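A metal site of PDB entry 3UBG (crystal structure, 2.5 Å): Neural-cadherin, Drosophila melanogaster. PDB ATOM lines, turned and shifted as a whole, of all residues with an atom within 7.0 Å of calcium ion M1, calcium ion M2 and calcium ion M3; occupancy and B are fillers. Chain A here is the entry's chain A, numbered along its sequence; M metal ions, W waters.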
ATOM      1  N   GLU A  13     -20.161 -23.086  33.937  1.00  0.00           N
ATOM      2  CA  GLU A  13     -20.102 -24.548  33.954  1.00  0.00           C
ATOM      3  C   GLU A  13     -19.159 -25.038  35.058  1.00  0.00           C
ATOM      4  O   GLU A  13     -19.317 -26.146  35.592  1.00  0.00           O
ATOM      5  CB  GLU A  13     -19.683 -25.096  32.596  1.00  0.00           C
ATOM      6  CG  GLU A  13     -18.277 -24.706  32.185  1.00  0.00           C
ATOM      7  CD  GLU A  13     -17.911 -25.137  30.771  1.00  0.00           C
ATOM      8  OE1 GLU A  13     -17.214 -24.362  30.100  1.00  0.00           O
ATOM      9  OE2 GLU A  13     -18.324 -26.235  30.323  1.00  0.00           O
ATOM     10  N   TRP A  58     -21.277 -30.188  35.189  1.00  0.00           N
ATOM     11  CA  TRP A  58     -21.783 -29.305  34.176  1.00  0.00           C
ATOM     12  C   TRP A  58     -20.783 -29.167  33.045  1.00  0.00           C
ATOM     13  O   TRP A  58     -19.569 -29.179  33.278  1.00  0.00           O
ATOM     14  CB  TRP A  58     -22.147 -27.962  34.801  1.00  0.00           C
ATOM     15  CG  TRP A  58     -23.400 -28.044  35.655  1.00  0.00           C
ATOM     16  CD1 TRP A  58     -24.196 -29.142  35.838  1.00  0.00           C
ATOM     17  CD2 TRP A  58     -23.965 -27.003  36.447  1.00  0.00           C
ATOM     18  NE1 TRP A  58     -25.242 -28.837  36.674  1.00  0.00           N
ATOM     19  CE2 TRP A  58     -25.126 -27.529  37.066  1.00  0.00           C
ATOM     20  CE3 TRP A  58     -23.616 -25.667  36.679  1.00  0.00           C
ATOM     21  CZ2 TRP A  58     -25.940 -26.754  37.907  1.00  0.00           C
ATOM     22  CZ3 TRP A  58     -24.435 -24.894  37.528  1.00  0.00           C
ATOM     23  CH2 TRP A  58     -25.584 -25.444  38.124  1.00  0.00           C
ATOM     24  N   ASP A  59     -21.292 -29.050  31.820  1.00  0.00           N
ATOM     25  CA  ASP A  59     -20.455 -28.993  30.642  1.00  0.00           C
ATOM     26  C   ASP A  59     -21.152 -28.185  29.547  1.00  0.00           C
ATOM     27  O   ASP A  59     -22.068 -28.668  28.874  1.00  0.00           O
ATOM     28  CB  ASP A  59     -20.081 -30.403  30.167  1.00  0.00           C
ATOM     29  CG  ASP A  59     -19.195 -30.414  28.917  1.00  0.00           C
ATOM     30  OD1 ASP A  59     -18.638 -29.368  28.528  1.00  0.00           O
ATOM     31  OD2 ASP A  59     -19.066 -31.497  28.326  1.00  0.00           O
ATOM     32  N   TYR A  60     -20.697 -26.938  29.408  1.00  0.00           N
ATOM     33  CA  TYR A  60     -21.208 -25.992  28.443  1.00  0.00           C
ATOM     34  C   TYR A  60     -21.125 -26.554  27.012  1.00  0.00           C
ATOM     35  O   TYR A  60     -22.021 -26.340  26.198  1.00  0.00           O
ATOM     36  CB  TYR A  60     -20.401 -24.698  28.567  1.00  0.00           C
ATOM     37  CG  TYR A  60     -20.837 -23.593  27.622  1.00  0.00           C
ATOM     38  CD1 TYR A  60     -21.772 -22.640  27.994  1.00  0.00           C
ATOM     39  CD2 TYR A  60     -20.280 -23.503  26.342  1.00  0.00           C
ATOM     40  CE1 TYR A  60     -22.160 -21.626  27.121  1.00  0.00           C
ATOM     41  CE2 TYR A  60     -20.658 -22.520  25.477  1.00  0.00           C
ATOM     42  CZ  TYR A  60     -21.603 -21.590  25.851  1.00  0.00           C
ATOM     43  OH  TYR A  60     -21.952 -20.603  24.945  1.00  0.00           O
ATOM     44  N   GLU A  61     -20.059 -27.296  26.712  1.00  0.00           N
ATOM     45  CA  GLU A  61     -19.919 -27.950  25.426  1.00  0.00           C
ATOM     46  C   GLU A  61     -21.000 -29.001  25.128  1.00  0.00           C
ATOM     47  O   GLU A  61     -21.378 -29.175  23.980  1.00  0.00           O
ATOM     48  CB  GLU A  61     -18.510 -28.546  25.259  1.00  0.00           C
ATOM     49  CG  GLU A  61     -17.432 -27.507  25.000  1.00  0.00           C
ATOM     50  CD  GLU A  61     -17.258 -26.497  26.132  1.00  0.00           C
ATOM     51  OE1 GLU A  61     -17.265 -26.914  27.317  1.00  0.00           O
ATOM     52  OE2 GLU A  61     -17.124 -25.278  25.856  1.00  0.00           O
ATOM     53  N   GLU A  62     -21.516 -29.694  26.120  1.00  0.00           N
ATOM     54  CA  GLU A  62     -22.571 -30.650  25.824  1.00  0.00           C
ATOM     55  C   GLU A  62     -24.007 -30.103  25.838  1.00  0.00           C
ATOM     56  O   GLU A  62     -24.928 -30.793  25.423  1.00  0.00           O
ATOM     57  CB  GLU A  62     -22.469 -31.902  26.710  1.00  0.00           C
ATOM     58  CG  GLU A  62     -21.223 -32.757  26.453  1.00  0.00           C
ATOM     59  CD  GLU A  62     -20.877 -32.872  24.979  1.00  0.00           C
ATOM     60  OE1 GLU A  62     -21.796 -33.114  24.157  1.00  0.00           O
ATOM     61  OE2 GLU A  62     -19.681 -32.706  24.636  1.00  0.00           O
ATOM     62  N   LYS A  97     -22.645 -20.714  31.737  1.00  0.00           N
ATOM     63  CA  LYS A  97     -21.657 -19.864  31.108  1.00  0.00           C
ATOM     64  C   LYS A  97     -20.379 -20.629  30.809  1.00  0.00           C
ATOM     65  O   LYS A  97     -19.932 -21.436  31.614  1.00  0.00           O
ATOM     66  CB  LYS A  97     -21.374 -18.667  32.008  1.00  0.00           C
ATOM     67  CG  LYS A  97     -22.494 -17.653  31.967  1.00  0.00           C
ATOM     68  CD  LYS A  97     -22.182 -16.491  32.839  1.00  0.00           C
ATOM     69  CE  LYS A  97     -22.474 -16.826  34.265  1.00  0.00           C
ATOM     70  NZ  LYS A  97     -22.096 -15.722  35.157  1.00  0.00           N
ATOM     71  N   ASP A  98     -19.810 -20.375  29.644  1.00  0.00           N
ATOM     72  CA  ASP A  98     -18.638 -21.094  29.198  1.00  0.00           C
ATOM     73  C   ASP A  98     -17.389 -20.665  29.961  1.00  0.00           C
ATOM     74  O   ASP A  98     -17.166 -19.481  30.182  1.00  0.00           O
ATOM     75  CB  ASP A  98     -18.398 -20.851  27.711  1.00  0.00           C
ATOM     76  CG  ASP A  98     -17.176 -21.567  27.199  1.00  0.00           C
ATOM     77  OD1 ASP A  98     -17.071 -22.766  27.490  1.00  0.00           O
ATOM     78  OD2 ASP A  98     -16.317 -20.944  26.540  1.00  0.00           O
ATOM     79  N   VAL A  99     -16.573 -21.647  30.337  1.00  0.00           N
ATOM     80  CA  VAL A  99     -15.270 -21.423  30.916  1.00  0.00           C
ATOM     81  C   VAL A  99     -14.270 -22.150  30.010  1.00  0.00           C
ATOM     82  O   VAL A  99     -14.616 -23.102  29.333  1.00  0.00           O
ATOM     83  CB  VAL A  99     -15.222 -21.941  32.392  1.00  0.00           C
ATOM     84  CG1 VAL A  99     -13.807 -22.052  32.877  1.00  0.00           C
ATOM     85  CG2 VAL A  99     -16.019 -21.027  33.333  1.00  0.00           C
ATOM     86  N   ASN A 100     -13.033 -21.695  29.955  1.00  0.00           N
ATOM     87  CA  ASN A 100     -12.083 -22.351  29.075  1.00  0.00           C
ATOM     88  C   ASN A 100     -11.535 -23.596  29.756  1.00  0.00           C
ATOM     89  O   ASN A 100     -10.656 -23.509  30.611  1.00  0.00           O
ATOM     90  CB  ASN A 100     -10.955 -21.393  28.695  1.00  0.00           C
ATOM     91  CG  ASN A 100     -10.173 -21.859  27.475  1.00  0.00           C
ATOM     92  OD1 ASN A 100      -9.858 -23.033  27.338  1.00  0.00           O
ATOM     93  ND2 ASN A 100      -9.822 -20.928  26.607  1.00  0.00           N
ATOM     94  N   ASP A 101     -12.056 -24.752  29.375  1.00  0.00           N
ATOM     95  CA  ASP A 101     -11.832 -25.959  30.151  1.00  0.00           C
ATOM     96  C   ASP A 101     -11.752 -27.221  29.296  1.00  0.00           C
ATOM     97  O   ASP A 101     -11.793 -28.334  29.819  1.00  0.00           O
ATOM     98  CB  ASP A 101     -12.928 -26.109  31.207  1.00  0.00           C
ATOM     99  CG  ASP A 101     -14.260 -26.530  30.623  1.00  0.00           C
ATOM    100  OD1 ASP A 101     -14.478 -26.317  29.410  1.00  0.00           O
ATOM    101  OD2 ASP A 101     -15.110 -27.069  31.365  1.00  0.00           O
ATOM    102  N   GLU A 102     -11.668 -27.055  27.986  1.00  0.00           N
ATOM    103  CA  GLU A 102     -11.516 -28.203  27.092  1.00  0.00           C
ATOM    104  C   GLU A 102     -10.220 -28.123  26.295  1.00  0.00           C
ATOM    105  O   GLU A 102      -9.849 -27.072  25.788  1.00  0.00           O
ATOM    106  CB  GLU A 102     -12.719 -28.323  26.152  1.00  0.00           C
ATOM    107  CG  GLU A 102     -14.052 -28.399  26.885  1.00  0.00           C
ATOM    108  CD  GLU A 102     -14.135 -29.589  27.829  1.00  0.00           C
ATOM    109  OE1 GLU A 102     -13.269 -30.489  27.768  1.00  0.00           O
ATOM    110  OE2 GLU A 102     -15.075 -29.653  28.629  1.00  0.00           O
ATOM    111  N   PRO A 103      -9.492 -29.234  26.191  1.00  0.00           N
ATOM    112  CA  PRO A 103      -8.218 -29.185  25.467  1.00  0.00           C
ATOM    113  C   PRO A 103      -8.412 -29.037  23.952  1.00  0.00           C
ATOM    114  O   PRO A 103      -9.457 -29.437  23.429  1.00  0.00           O
ATOM    115  CB  PRO A 103      -7.582 -30.540  25.809  1.00  0.00           C
ATOM    116  CG  PRO A 103      -8.754 -31.456  26.074  1.00  0.00           C
ATOM    117  CD  PRO A 103      -9.790 -30.570  26.735  1.00  0.00           C
ATOM    118  N   PRO A 104      -7.421 -28.453  23.248  1.00  0.00           N
ATOM    119  CA  PRO A 104      -7.439 -28.421  21.783  1.00  0.00           C
ATOM    120  C   PRO A 104      -7.122 -29.771  21.143  1.00  0.00           C
ATOM    121  O   PRO A 104      -6.572 -30.660  21.786  1.00  0.00           O
ATOM    122  CB  PRO A 104      -6.318 -27.443  21.450  1.00  0.00           C
ATOM    123  CG  PRO A 104      -5.366 -27.594  22.597  1.00  0.00           C
ATOM    124  CD  PRO A 104      -6.256 -27.739  23.794  1.00  0.00           C
ATOM    125  N   ASP A 134     -10.232 -25.866  19.066  1.00  0.00           N
ATOM    126  CA  ASP A 134     -10.461 -25.930  20.498  1.00  0.00           C
ATOM    127  C   ASP A 134     -11.931 -25.605  20.763  1.00  0.00           C
ATOM    128  O   ASP A 134     -12.471 -24.678  20.182  1.00  0.00           O
ATOM    129  CB  ASP A 134      -9.552 -24.941  21.211  1.00  0.00           C
ATOM    130  CG  ASP A 134      -9.716 -24.985  22.705  1.00  0.00           C
ATOM    131  OD1 ASP A 134     -10.790 -24.573  23.230  1.00  0.00           O
ATOM    132  OD2 ASP A 134      -8.751 -25.441  23.346  1.00  0.00           O
ATOM    133  N   PRO A 135     -12.583 -26.370  21.644  1.00  0.00           N
ATOM    134  CA  PRO A 135     -14.027 -26.328  21.852  1.00  0.00           C
ATOM    135  C   PRO A 135     -14.525 -25.076  22.559  1.00  0.00           C
ATOM    136  O   PRO A 135     -15.677 -24.736  22.404  1.00  0.00           O
ATOM    137  CB  PRO A 135     -14.303 -27.565  22.720  1.00  0.00           C
ATOM    138  CG  PRO A 135     -13.074 -28.416  22.605  1.00  0.00           C
ATOM    139  CD  PRO A 135     -11.944 -27.467  22.408  1.00  0.00           C
ATOM    140  N   ASP A 136     -13.683 -24.381  23.303  1.00  0.00           N
ATOM    141  CA  ASP A 136     -14.170 -23.233  24.059  1.00  0.00           C
ATOM    142  C   ASP A 136     -14.434 -22.025  23.159  1.00  0.00           C
ATOM    143  O   ASP A 136     -13.929 -21.959  22.042  1.00  0.00           O
ATOM    144  CB  ASP A 136     -13.200 -22.909  25.193  1.00  0.00           C
ATOM    145  CG  ASP A 136     -12.955 -24.123  26.081  1.00  0.00           C
ATOM    146  OD1 ASP A 136     -13.894 -24.855  26.373  1.00  0.00           O
ATOM    147  OD2 ASP A 136     -11.813 -24.390  26.468  1.00  0.00           O
ATOM    148  N   THR A 137     -15.254 -21.093  23.632  1.00  0.00           N
ATOM    149  CA  THR A 137     -15.547 -19.879  22.868  1.00  0.00           C
ATOM    150  C   THR A 137     -14.352 -18.931  22.935  1.00  0.00           C
ATOM    151  O   THR A 137     -14.258 -17.999  22.152  1.00  0.00           O
ATOM    152  CB  THR A 137     -16.795 -19.136  23.419  1.00  0.00           C
ATOM    153  OG1 THR A 137     -16.520 -18.589  24.721  1.00  0.00           O
ATOM    154  CG2 THR A 137     -17.998 -20.064  23.526  1.00  0.00           C
ATOM    155  N   ASP A 138     -13.426 -19.220  23.838  1.00  0.00           N
ATOM    156  CA  ASP A 138     -12.405 -18.285  24.295  1.00  0.00           C
ATOM    157  C   ASP A 138     -10.964 -18.788  24.041  1.00  0.00           C
ATOM    158  O   ASP A 138     -10.045 -18.501  24.817  1.00  0.00           O
ATOM    159  CB  ASP A 138     -12.646 -18.081  25.788  1.00  0.00           C
ATOM    160  CG  ASP A 138     -11.664 -17.113  26.417  1.00  0.00           C
ATOM    161  OD1 ASP A 138     -11.109 -16.246  25.707  1.00  0.00           O
ATOM    162  OD2 ASP A 138     -11.475 -17.219  27.664  1.00  0.00           O
ATOM    163  N   HIS A 139     -10.758 -19.525  22.964  1.00  0.00           N
ATOM    164  CA  HIS A 139      -9.451 -20.154  22.714  1.00  0.00           C
ATOM    165  C   HIS A 139      -8.378 -19.216  22.174  1.00  0.00           C
ATOM    166  O   HIS A 139      -8.647 -18.141  21.665  1.00  0.00           O
ATOM    167  CB  HIS A 139      -9.629 -21.288  21.721  1.00  0.00           C
ATOM    168  CG  HIS A 139     -10.300 -20.871  20.463  1.00  0.00           C
ATOM    169  ND1 HIS A 139      -9.649 -20.191  19.469  1.00  0.00           N
ATOM    170  CD2 HIS A 139     -11.581 -21.021  20.052  1.00  0.00           C
ATOM    171  CE1 HIS A 139     -10.495 -19.944  18.481  1.00  0.00           C
ATOM    172  NE2 HIS A 139     -11.673 -20.446  18.809  1.00  0.00           N
ATOM    173  N   ASN A 140      -7.132 -19.658  22.294  1.00  0.00           N
ATOM    174  CA  ASN A 140      -5.970 -18.908  21.846  1.00  0.00           C
ATOM    175  C   ASN A 140      -4.845 -19.880  21.520  1.00  0.00           C
ATOM    176  O   ASN A 140      -3.992 -20.154  22.366  1.00  0.00           O
ATOM    177  CB  ASN A 140      -5.541 -17.930  22.941  1.00  0.00           C
ATOM    178  CG  ASN A 140      -4.297 -17.125  22.572  1.00  0.00           C
ATOM    179  OD1 ASN A 140      -4.056 -16.819  21.400  1.00  0.00           O
ATOM    180  ND2 ASN A 140      -3.511 -16.766  23.585  1.00  0.00           N
ATOM    181  N   ASP A 185      -3.793 -24.339  23.966  1.00  0.00           N
ATOM    182  CA  ASP A 185      -4.703 -23.221  24.116  1.00  0.00           C
ATOM    183  C   ASP A 185      -4.141 -22.398  25.264  1.00  0.00           C
ATOM    184  O   ASP A 185      -4.240 -22.796  26.429  1.00  0.00           O
ATOM    185  CB  ASP A 185      -6.138 -23.685  24.389  1.00  0.00           C
ATOM    186  CG  ASP A 185      -7.084 -22.523  24.692  1.00  0.00           C
ATOM    187  OD1 ASP A 185      -6.668 -21.352  24.561  1.00  0.00           O
ATOM    188  OD2 ASP A 185      -8.260 -22.781  25.035  1.00  0.00           O
ATOM    189  N   ASN A 187      -5.160 -19.822  26.499  1.00  0.00           N
ATOM    190  CA  ASN A 187      -6.185 -19.229  27.347  1.00  0.00           C
ATOM    191  C   ASN A 187      -6.725 -20.178  28.414  1.00  0.00           C
ATOM    192  O   ASN A 187      -7.652 -19.818  29.129  1.00  0.00           O
ATOM    193  CB  ASN A 187      -7.351 -18.717  26.513  1.00  0.00           C
ATOM    194  CG  ASN A 187      -7.113 -17.332  25.997  1.00  0.00           C
ATOM    195  OD1 ASN A 187      -6.030 -16.770  26.176  1.00  0.00           O
ATOM    196  ND2 ASN A 187      -8.116 -16.765  25.330  1.00  0.00           N
ATOM    197  N   GLY A 188      -6.155 -21.377  28.507  1.00  0.00           N
ATOM    198  CA  GLY A 188      -6.648 -22.382  29.445  1.00  0.00           C
ATOM    199  C   GLY A 188      -5.536 -23.055  30.235  1.00  0.00           C
ATOM    200  O   GLY A 188      -4.829 -23.925  29.707  1.00  0.00           O
ATOM    201  N   GLN A 196      -3.593 -26.244  28.521  1.00  0.00           N
ATOM    202  CA  GLN A 196      -4.255 -27.323  27.799  1.00  0.00           C
ATOM    203  C   GLN A 196      -3.564 -27.624  26.458  1.00  0.00           C
ATOM    204  O   GLN A 196      -3.168 -26.713  25.734  1.00  0.00           O
ATOM    205  CB  GLN A 196      -5.710 -26.991  27.521  1.00  0.00           C
ATOM    206  CG  GLN A 196      -6.533 -26.610  28.721  1.00  0.00           C
ATOM    207  CD  GLN A 196      -7.653 -25.672  28.315  1.00  0.00           C
ATOM    208  OE1 GLN A 196      -7.670 -25.162  27.199  1.00  0.00           O
ATOM    209  NE2 GLN A 196      -8.585 -25.424  29.219  1.00  0.00           N
HETATM  210 CA    CA M   1     -16.721 -28.020  29.504  1.00  0.00          CA
HETATM  211 CA    CA M   2      -9.637 -24.729  25.528  1.00  0.00          CA
HETATM  212 CA    CA M   3     -15.804 -24.687  27.996  1.00  0.00          CA
HETATM  213  O   HOH W   1     -17.304 -29.610  31.670  1.00  0.00           O
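N of Tyr 60 lies close to OE2 of Glu 13, at 2.6 Å. OD1 of Asp 185 is in hydrogen-bond range of N of Asn 187, at 2.9 Å. The side-chain carboxylate (OD2) of Asp 98 lies within hydrogen-bond range of the side-chain hydroxyl (OG1) of Thr 137 (3.0 Å). The side-chain amide nitrogen of Asn 100 lies within hydrogen-bond range of the backbone carbonyl oxygen of Asp 138, at 3.0 Å. N of Glu 13 sits at hydrogen-bond distance from O of Lys 97, at 2.9 Å. OD1 of Asp 185 sits at hydrogen-bond distance from N of Asn 140, 2.9 Å away. N of Gln 196 is in hydrogen-bond range of O of Gly 188 (2.9 Å).
Within 4 Å of calcium ion M2: Asn 100, Glu 102, Asp 134, Asp 136, Asp 185 and Gln 196. The nearest printed residue that does not touch calcium ion M2 is Asp 101 (4.5 Å).
Along chain A the residues within 4 Å of calcium ion M3 span positions 13 to 136. The nearest printed residue that does not touch calcium ion M3 is Glu 102 (4.3 Å).
Calcium ion M1 is bound by OE2 of Glu 102 (2.5 Å), OE1 of Glu 61 (2.5 Å), OE2 of Glu 13 (2.5 Å), OD1 of Asp 59 (2.5 Å), OD2 of Asp 101 (2.6 Å), water W1 (2.7 Å) and OD1 of Asp 101 (2.8 Å).
Calcium ion M2 is bound by the backbone carbonyl oxygen (O) of Glu 102, at 2.4 Å. The side-chain carboxylate (OD2) of Asp 136 binds calcium ion M2, at 2.4 Å. The side-chain carboxylate (OD2) of Asp 185 binds calcium ion M2, at 2.4 Å. OD2 of Asp 134 binds calcium ion M2 (2.5 Å). The side-chain amide oxygen (OD1) of Asn 100 is bound to calcium ion M2 (2.5 Å). Calcium ion M2 is bound by OD1 of Asp 134 (2.6 Å). OE1 of Gln 196 is bound to calcium ion M2.
Calcium ion M3 is bound by the side-chain carboxylate (OD1) of Asp 98 (2.4 Å), the backbone carbonyl oxygen (O) of Val 99 (2.4 Å), the side-chain carboxylate (OD1) of Asp 136 (2.5 Å), the side-chain carboxylate (OD1) of Asp 101 (2.5 Å), the side-chain carboxylate (OE1) of Glu 13 (2.6 Å), the side-chain carboxylate (OE2) of Glu 61 (2.6 Å) and the side-chain carboxylate (OE1) of Glu 61 (2.7 Å). Calcium ion M3 has seven donor atoms within binding distance.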
